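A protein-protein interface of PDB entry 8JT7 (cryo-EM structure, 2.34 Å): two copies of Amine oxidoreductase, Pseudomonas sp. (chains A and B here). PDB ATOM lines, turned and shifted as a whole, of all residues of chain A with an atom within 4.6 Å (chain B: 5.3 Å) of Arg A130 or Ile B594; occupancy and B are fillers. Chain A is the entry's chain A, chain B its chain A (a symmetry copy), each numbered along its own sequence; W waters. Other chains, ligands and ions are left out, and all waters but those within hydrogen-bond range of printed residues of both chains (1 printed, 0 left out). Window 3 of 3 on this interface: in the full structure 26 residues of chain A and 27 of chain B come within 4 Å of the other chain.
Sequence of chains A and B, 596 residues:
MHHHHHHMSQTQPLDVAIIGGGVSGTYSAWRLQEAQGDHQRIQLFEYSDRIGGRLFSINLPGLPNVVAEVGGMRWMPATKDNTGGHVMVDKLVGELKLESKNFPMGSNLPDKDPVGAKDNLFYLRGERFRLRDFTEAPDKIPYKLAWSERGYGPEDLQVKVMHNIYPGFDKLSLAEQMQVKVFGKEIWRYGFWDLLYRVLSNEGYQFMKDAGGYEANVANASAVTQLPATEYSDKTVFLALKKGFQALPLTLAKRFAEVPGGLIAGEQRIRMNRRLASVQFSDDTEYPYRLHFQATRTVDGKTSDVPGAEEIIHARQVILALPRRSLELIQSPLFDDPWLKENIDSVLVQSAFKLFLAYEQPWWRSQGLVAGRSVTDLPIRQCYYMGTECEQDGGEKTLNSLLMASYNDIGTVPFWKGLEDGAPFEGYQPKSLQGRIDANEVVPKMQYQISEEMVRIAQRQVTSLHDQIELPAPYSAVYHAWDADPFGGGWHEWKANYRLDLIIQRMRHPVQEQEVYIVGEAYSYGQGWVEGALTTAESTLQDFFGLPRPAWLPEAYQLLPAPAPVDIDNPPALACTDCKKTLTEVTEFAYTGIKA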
ATOM      1  N   LYS A 118     -15.252 -16.696  16.882  1.00  0.00           N
ATOM      2  CA  LYS A 118     -16.010 -16.187  18.006  1.00  0.00           C
ATOM      3  C   LYS A 118     -15.299 -16.425  19.324  1.00  0.00           C
ATOM      4  O   LYS A 118     -15.526 -15.685  20.262  1.00  0.00           O
ATOM      5  CB  LYS A 118     -17.373 -16.867  18.116  1.00  0.00           C
ATOM      6  CG  LYS A 118     -18.407 -16.310  17.174  1.00  0.00           C
ATOM      7  CD  LYS A 118     -19.781 -16.832  17.438  1.00  0.00           C
ATOM      8  CE  LYS A 118     -19.868 -18.347  17.412  1.00  0.00           C
ATOM      9  NZ  LYS A 118     -19.995 -18.831  16.015  1.00  0.00           N
ATOM     10  N   ASP A 119     -14.464 -17.451  19.398  1.00  0.00           N
ATOM     11  CA  ASP A 119     -13.772 -17.763  20.628  1.00  0.00           C
ATOM     12  C   ASP A 119     -12.344 -17.200  20.689  1.00  0.00           C
ATOM     13  O   ASP A 119     -11.626 -17.461  21.649  1.00  0.00           O
ATOM     14  CB  ASP A 119     -13.723 -19.288  20.802  1.00  0.00           C
ATOM     15  CG  ASP A 119     -15.071 -19.859  21.237  1.00  0.00           C
ATOM     16  OD1 ASP A 119     -15.893 -19.079  21.785  1.00  0.00           O
ATOM     17  OD2 ASP A 119     -15.312 -21.083  21.018  1.00  0.00           O
ATOM     18  N   ASN A 120     -11.922 -16.413  19.703  1.00  0.00           N
ATOM     19  CA  ASN A 120     -10.570 -15.873  19.692  1.00  0.00           C
ATOM     20  C   ASN A 120     -10.462 -14.768  20.738  1.00  0.00           C
ATOM     21  O   ASN A 120     -11.476 -14.182  21.112  1.00  0.00           O
ATOM     22  CB  ASN A 120     -10.183 -15.424  18.291  1.00  0.00           C
ATOM     23  CG  ASN A 120      -9.898 -16.585  17.357  1.00  0.00           C
ATOM     24  OD1 ASN A 120     -10.357 -17.708  17.544  1.00  0.00           O
ATOM     25  ND2 ASN A 120      -9.134 -16.350  16.320  1.00  0.00           N
ATOM     26  N   LEU A 121      -9.247 -14.516  21.234  1.00  0.00           N
ATOM     27  CA  LEU A 121      -9.104 -13.820  22.495  1.00  0.00           C
ATOM     28  C   LEU A 121      -8.835 -12.344  22.256  1.00  0.00           C
ATOM     29  O   LEU A 121      -8.330 -11.958  21.223  1.00  0.00           O
ATOM     30  CB  LEU A 121      -7.934 -14.370  23.308  1.00  0.00           C
ATOM     31  CG  LEU A 121      -7.973 -15.864  23.584  1.00  0.00           C
ATOM     32  CD1 LEU A 121      -6.751 -16.255  24.370  1.00  0.00           C
ATOM     33  CD2 LEU A 121      -9.226 -16.226  24.322  1.00  0.00           C
ATOM     34  N   PHE A 122      -9.278 -11.558  23.224  1.00  0.00           N
ATOM     35  CA  PHE A 122      -8.876 -10.191  23.419  1.00  0.00           C
ATOM     36  C   PHE A 122      -8.390 -10.024  24.840  1.00  0.00           C
ATOM     37  O   PHE A 122      -8.965 -10.563  25.778  1.00  0.00           O
ATOM     38  CB  PHE A 122     -10.026  -9.235  23.210  1.00  0.00           C
ATOM     39  CG  PHE A 122     -10.420  -9.124  21.767  1.00  0.00           C
ATOM     40  CD1 PHE A 122     -11.245 -10.074  21.192  1.00  0.00           C
ATOM     41  CD2 PHE A 122      -9.942  -8.092  20.990  1.00  0.00           C
ATOM     42  CE1 PHE A 122     -11.584  -9.980  19.861  1.00  0.00           C
ATOM     43  CE2 PHE A 122     -10.269  -8.011  19.650  1.00  0.00           C
ATOM     44  CZ  PHE A 122     -11.095  -8.935  19.099  1.00  0.00           C
ATOM     45  N   PHE A 129     -11.664 -11.087  27.189  1.00  0.00           N
ATOM     46  CA  PHE A 129     -12.945 -11.426  26.659  1.00  0.00           C
ATOM     47  C   PHE A 129     -12.691 -12.043  25.306  1.00  0.00           C
ATOM     48  O   PHE A 129     -11.559 -12.163  24.899  1.00  0.00           O
ATOM     49  CB  PHE A 129     -13.880 -10.230  26.570  1.00  0.00           C
ATOM     50  CG  PHE A 129     -13.358  -9.084  25.753  1.00  0.00           C
ATOM     51  CD1 PHE A 129     -12.517  -8.140  26.307  1.00  0.00           C
ATOM     52  CD2 PHE A 129     -13.671  -8.989  24.407  1.00  0.00           C
ATOM     53  CE1 PHE A 129     -12.045  -7.082  25.540  1.00  0.00           C
ATOM     54  CE2 PHE A 129     -13.195  -7.936  23.641  1.00  0.00           C
ATOM     55  CZ  PHE A 129     -12.378  -6.987  24.209  1.00  0.00           C
ATOM     56  N   ARG A 130     -13.748 -12.561  24.698  1.00  0.00           N
ATOM     57  CA  ARG A 130     -13.609 -13.238  23.435  1.00  0.00           C
ATOM     58  C   ARG A 130     -14.393 -12.441  22.437  1.00  0.00           C
ATOM     59  O   ARG A 130     -15.112 -11.548  22.854  1.00  0.00           O
ATOM     60  CB  ARG A 130     -14.133 -14.652  23.507  1.00  0.00           C
ATOM     61  CG  ARG A 130     -13.261 -15.553  24.332  1.00  0.00           C
ATOM     62  CD  ARG A 130     -13.967 -16.870  24.450  1.00  0.00           C
ATOM     63  NE  ARG A 130     -13.455 -17.530  25.639  1.00  0.00           N
ATOM     64  CZ  ARG A 130     -12.352 -18.240  25.626  1.00  0.00           C
ATOM     65  NH1 ARG A 130     -11.728 -18.474  24.472  1.00  0.00           N
ATOM     66  NH2 ARG A 130     -11.929 -18.775  26.757  1.00  0.00           N
ATOM     67  N   LEU A 131     -14.163 -12.726  21.158  1.00  0.00           N
ATOM     68  CA  LEU A 131     -14.700 -11.898  20.099  1.00  0.00           C
ATOM     69  C   LEU A 131     -16.228 -11.816  20.176  1.00  0.00           C
ATOM     70  O   LEU A 131     -16.810 -10.743  20.004  1.00  0.00           O
ATOM     71  CB  LEU A 131     -14.278 -12.480  18.760  1.00  0.00           C
ATOM     72  CG  LEU A 131     -14.660 -11.632  17.530  1.00  0.00           C
ATOM     73  CD1 LEU A 131     -13.489 -11.451  16.603  1.00  0.00           C
ATOM     74  CD2 LEU A 131     -15.779 -12.282  16.761  1.00  0.00           C
ATOM     75  N   ARG A 132     -16.865 -12.940  20.479  1.00  0.00           N
ATOM     76  CA  ARG A 132     -18.318 -13.015  20.584  1.00  0.00           C
ATOM     77  C   ARG A 132     -18.870 -12.075  21.651  1.00  0.00           C
ATOM     78  O   ARG A 132     -20.042 -11.743  21.625  1.00  0.00           O
ATOM     79  CB  ARG A 132     -18.734 -14.448  20.877  1.00  0.00           C
ATOM     80  CG  ARG A 132     -18.556 -14.869  22.312  1.00  0.00           C
ATOM     81  CD  ARG A 132     -18.379 -16.368  22.419  1.00  0.00           C
ATOM     82  NE  ARG A 132     -19.559 -17.063  21.946  1.00  0.00           N
ATOM     83  CZ  ARG A 132     -19.560 -18.189  21.249  1.00  0.00           C
ATOM     84  NH1 ARG A 132     -18.438 -18.757  20.843  1.00  0.00           N
ATOM     85  NH2 ARG A 132     -20.714 -18.759  20.961  1.00  0.00           N
ATOM     86  N   ASP A 133     -18.027 -11.578  22.553  1.00  0.00           N
ATOM     87  CA  ASP A 133     -18.531 -10.741  23.621  1.00  0.00           C
ATOM     88  C   ASP A 133     -18.811  -9.320  23.140  1.00  0.00           C
ATOM     89  O   ASP A 133     -19.435  -8.547  23.854  1.00  0.00           O
ATOM     90  CB  ASP A 133     -17.574 -10.725  24.805  1.00  0.00           C
ATOM     91  CG  ASP A 133     -17.481 -12.071  25.501  1.00  0.00           C
ATOM     92  OD1 ASP A 133     -18.567 -12.664  25.752  1.00  0.00           O
ATOM     93  OD2 ASP A 133     -16.335 -12.489  25.886  1.00  0.00           O
ATOM     94  N   PHE A 134     -18.366  -8.934  21.943  1.00  0.00           N
ATOM     95  CA  PHE A 134     -18.711  -7.595  21.461  1.00  0.00           C
ATOM     96  C   PHE A 134     -20.225  -7.440  21.276  1.00  0.00           C
ATOM     97  O   PHE A 134     -20.774  -6.372  21.500  1.00  0.00           O
ATOM     98  CB  PHE A 134     -18.048  -7.290  20.128  1.00  0.00           C
ATOM     99  CG  PHE A 134     -16.556  -7.121  20.197  1.00  0.00           C
ATOM    100  CD1 PHE A 134     -16.007  -6.123  20.970  1.00  0.00           C
ATOM    101  CD2 PHE A 134     -15.717  -7.889  19.396  1.00  0.00           C
ATOM    102  CE1 PHE A 134     -14.639  -5.942  21.005  1.00  0.00           C
ATOM    103  CE2 PHE A 134     -14.346  -7.715  19.447  1.00  0.00           C
ATOM    104  CZ  PHE A 134     -13.819  -6.741  20.250  1.00  0.00           C
ATOM    105  N   GLN A 367      -7.001 -24.660  24.054  1.00  0.00           N
ATOM    106  CA  GLN A 367      -7.641 -23.485  24.629  1.00  0.00           C
ATOM    107  C   GLN A 367      -8.863 -23.086  23.822  1.00  0.00           C
ATOM    108  O   GLN A 367      -9.455 -22.049  24.079  1.00  0.00           O
ATOM    109  CB  GLN A 367      -6.600 -22.365  24.652  1.00  0.00           C
ATOM    110  CG  GLN A 367      -5.304 -22.813  25.337  1.00  0.00           C
ATOM    111  CD  GLN A 367      -4.365 -21.714  25.773  1.00  0.00           C
ATOM    112  OE1 GLN A 367      -4.713 -20.528  25.800  1.00  0.00           O
ATOM    113  NE2 GLN A 367      -3.179 -22.122  26.203  1.00  0.00           N
ATOM    114  N   GLY A 368      -9.196 -23.876  22.797  1.00  0.00           N
ATOM    115  CA  GLY A 368     -10.274 -23.534  21.909  1.00  0.00           C
ATOM    116  C   GLY A 368      -9.838 -22.635  20.760  1.00  0.00           C
ATOM    117  O   GLY A 368     -10.693 -22.037  20.135  1.00  0.00           O
ATOM    118  N   TRP B 147      -9.346 -17.031  34.538  1.00  0.00           N
ATOM    119  CA  TRP B 147     -10.345 -16.775  33.543  1.00  0.00           C
ATOM    120  C   TRP B 147     -10.472 -17.971  32.603  1.00  0.00           C
ATOM    121  O   TRP B 147     -11.580 -18.301  32.217  1.00  0.00           O
ATOM    122  CB  TRP B 147      -9.930 -15.506  32.812  1.00  0.00           C
ATOM    123  CG  TRP B 147     -10.874 -15.108  31.739  1.00  0.00           C
ATOM    124  CD1 TRP B 147     -12.030 -14.424  31.883  1.00  0.00           C
ATOM    125  CD2 TRP B 147     -10.769 -15.433  30.352  1.00  0.00           C
ATOM    126  NE1 TRP B 147     -12.643 -14.277  30.675  1.00  0.00           N
ATOM    127  CE2 TRP B 147     -11.882 -14.869  29.714  1.00  0.00           C
ATOM    128  CE3 TRP B 147      -9.811 -16.074  29.590  1.00  0.00           C
ATOM    129  CZ2 TRP B 147     -12.056 -14.908  28.344  1.00  0.00           C
ATOM    130  CZ3 TRP B 147     -10.012 -16.166  28.237  1.00  0.00           C
ATOM    131  CH2 TRP B 147     -11.106 -15.591  27.629  1.00  0.00           C
ATOM    132  N   TYR B 152     -15.664 -25.213  34.125  1.00  0.00           N
ATOM    133  CA  TYR B 152     -15.448 -26.638  34.102  1.00  0.00           C
ATOM    134  C   TYR B 152     -15.702 -27.176  35.493  1.00  0.00           C
ATOM    135  O   TYR B 152     -15.362 -26.539  36.480  1.00  0.00           O
ATOM    136  CB  TYR B 152     -14.005 -27.005  33.724  1.00  0.00           C
ATOM    137  CG  TYR B 152     -13.572 -26.492  32.389  1.00  0.00           C
ATOM    138  CD1 TYR B 152     -13.820 -27.224  31.229  1.00  0.00           C
ATOM    139  CD2 TYR B 152     -12.981 -25.242  32.265  1.00  0.00           C
ATOM    140  CE1 TYR B 152     -13.454 -26.734  29.981  1.00  0.00           C
ATOM    141  CE2 TYR B 152     -12.608 -24.738  31.021  1.00  0.00           C
ATOM    142  CZ  TYR B 152     -12.859 -25.483  29.879  1.00  0.00           C
ATOM    143  OH  TYR B 152     -12.527 -24.974  28.654  1.00  0.00           O
ATOM    144  N   ALA B 590     -12.447 -27.961  24.574  1.00  0.00           N
ATOM    145  CA  ALA B 590     -12.247 -26.598  25.039  1.00  0.00           C
ATOM    146  C   ALA B 590     -13.532 -25.796  24.855  1.00  0.00           C
ATOM    147  O   ALA B 590     -13.903 -25.030  25.734  1.00  0.00           O
ATOM    148  CB  ALA B 590     -11.094 -25.947  24.329  1.00  0.00           C
ATOM    149  N   TYR B 591     -14.216 -26.013  23.737  1.00  0.00           N
ATOM    150  CA  TYR B 591     -15.483 -25.353  23.484  1.00  0.00           C
ATOM    151  C   TYR B 591     -16.534 -25.702  24.535  1.00  0.00           C
ATOM    152  O   TYR B 591     -17.390 -24.875  24.836  1.00  0.00           O
ATOM    153  CB  TYR B 591     -15.993 -25.737  22.101  1.00  0.00           C
ATOM    154  CG  TYR B 591     -15.216 -25.172  20.948  1.00  0.00           C
ATOM    155  CD1 TYR B 591     -14.314 -24.119  21.109  1.00  0.00           C
ATOM    156  CD2 TYR B 591     -15.383 -25.712  19.683  1.00  0.00           C
ATOM    157  CE1 TYR B 591     -13.621 -23.599  20.031  1.00  0.00           C
ATOM    158  CE2 TYR B 591     -14.661 -25.231  18.605  1.00  0.00           C
ATOM    159  CZ  TYR B 591     -13.796 -24.162  18.779  1.00  0.00           C
ATOM    160  OH  TYR B 591     -13.110 -23.689  17.712  1.00  0.00           O
ATOM    161  N   THR B 592     -16.450 -26.912  25.095  1.00  0.00           N
ATOM    162  CA  THR B 592     -17.351 -27.357  26.156  1.00  0.00           C
ATOM    163  C   THR B 592     -17.357 -26.377  27.329  1.00  0.00           C
ATOM    164  O   THR B 592     -18.411 -26.111  27.900  1.00  0.00           O
ATOM    165  CB  THR B 592     -16.989 -28.772  26.611  1.00  0.00           C
ATOM    166  OG1 THR B 592     -17.652 -29.653  25.706  1.00  0.00           O
ATOM    167  CG2 THR B 592     -17.354 -29.072  28.048  1.00  0.00           C
ATOM    168  N   GLY B 593     -16.188 -25.842  27.688  1.00  0.00           N
ATOM    169  CA  GLY B 593     -16.092 -24.933  28.820  1.00  0.00           C
ATOM    170  C   GLY B 593     -16.535 -23.519  28.484  1.00  0.00           C
ATOM    171  O   GLY B 593     -16.922 -22.788  29.397  1.00  0.00           O
ATOM    172  N   ILE B 594     -16.436 -23.142  27.194  1.00  0.00           N
ATOM    173  CA  ILE B 594     -16.513 -21.750  26.753  1.00  0.00           C
ATOM    174  C   ILE B 594     -17.979 -21.471  26.416  1.00  0.00           C
ATOM    175  O   ILE B 594     -18.550 -20.569  27.065  1.00  0.00           O
ATOM    176  CB  ILE B 594     -15.575 -21.444  25.552  1.00  0.00           C
ATOM    177  CG1 ILE B 594     -14.098 -21.700  25.864  1.00  0.00           C
ATOM    178  CG2 ILE B 594     -15.748 -20.021  25.022  1.00  0.00           C
ATOM    179  CD1 ILE B 594     -13.230 -21.896  24.627  1.00  0.00           C
HETATM  180  O   HOH W   1     -11.950 -21.460  17.981  1.00  0.00           O
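No position is printed for both chains.
The side-chain carboxylate (OD1) of Asp A119 lies within salt-bridge range of the guanidinium group (NH1) of Arg A132 (2.7 Å).
The backbone carbonyl oxygen (O) of Ala B590 is in hydrogen-bond range of the side-chain hydroxyl (OH) of Tyr B152 (3.2 Å).
The backbone carbonyl oxygen (O) of Asp A119 sits at hydrogen-bond distance from the guanidinium group (NH1) of Arg A130.
N of Arg A130 sits at hydrogen-bond distance from OD2 of Asp A133 (2.8 Å).
N of Phe A122 lies within hydrogen-bond range of O of Phe A129 (2.9 Å).
Water W1 bridges the side-chain hydroxyl of Tyr B591 and the backbone carbonyl oxygen of Gly A368.
Printed residues of chain A that touch a printed residue of chain B: Asp A119, Leu A121, Phe A129, Arg A130, Gln A367 and Gly A368.
Hydrophobic or aromatic side chains of chain A that line the printed part of chain B: Leu A121.
Along chain A the printed residues that touch a printed residue of chain B span positions 119 to 368.
Of the printed residues of chain A, Ile B594 touches Asp A119 (3.4 Å), Arg A130 (3.4 Å) and Gln A367 (3.8 Å).
Printed residues of chain B within 4 Å of Phe A129: Trp B147.
Of the printed residues of chain A, Trp B147 touches Leu A121 (3.9 Å), Phe A129 (3.97 Å) and Arg A130 (3.4 Å).
Of the printed residues of chain B, Gly A368 touches Ala B590 and Tyr B591.
Of the printed residues of chain B, Gln A367 touches Ala B590 and Ile B594.
Printed residues of chain A within 4 Å of Ala B590: Gln A367 (3.7 Å) and Gly A368 (3.2 Å).
Tyr B152 touches none of the printed residues of chain A.
Asn A120 touches none of the printed residues of chain B.
The nearest printed residue of chain B that does not touch Arg A130 is Tyr B152 (6.5 Å).
Asp A119 touches Tyr B591 (OD2 to CE1, 3.2 Å).
OD1 of Asp A119 touches CG2 of Ile B594, 3.4 Å away.
Leu A121 touches Trp B147 (CD2 to CH2, 3.9 Å).
Trp B147 touches Phe A129.
Arg A130 touches Trp B147 (NH2 to CH2, 3.4 Å).
Arg A130 touches Ile B594 (NE to CG2, 3.4 Å).
Ala B590 touches Gln A367.
Ile B594 touches Gln A367 (CD1 to O, 3.8 Å).
Ala B590 touches Gly A368 (CB to N, 3.2 Å).
Gly A368 touches Tyr B591.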
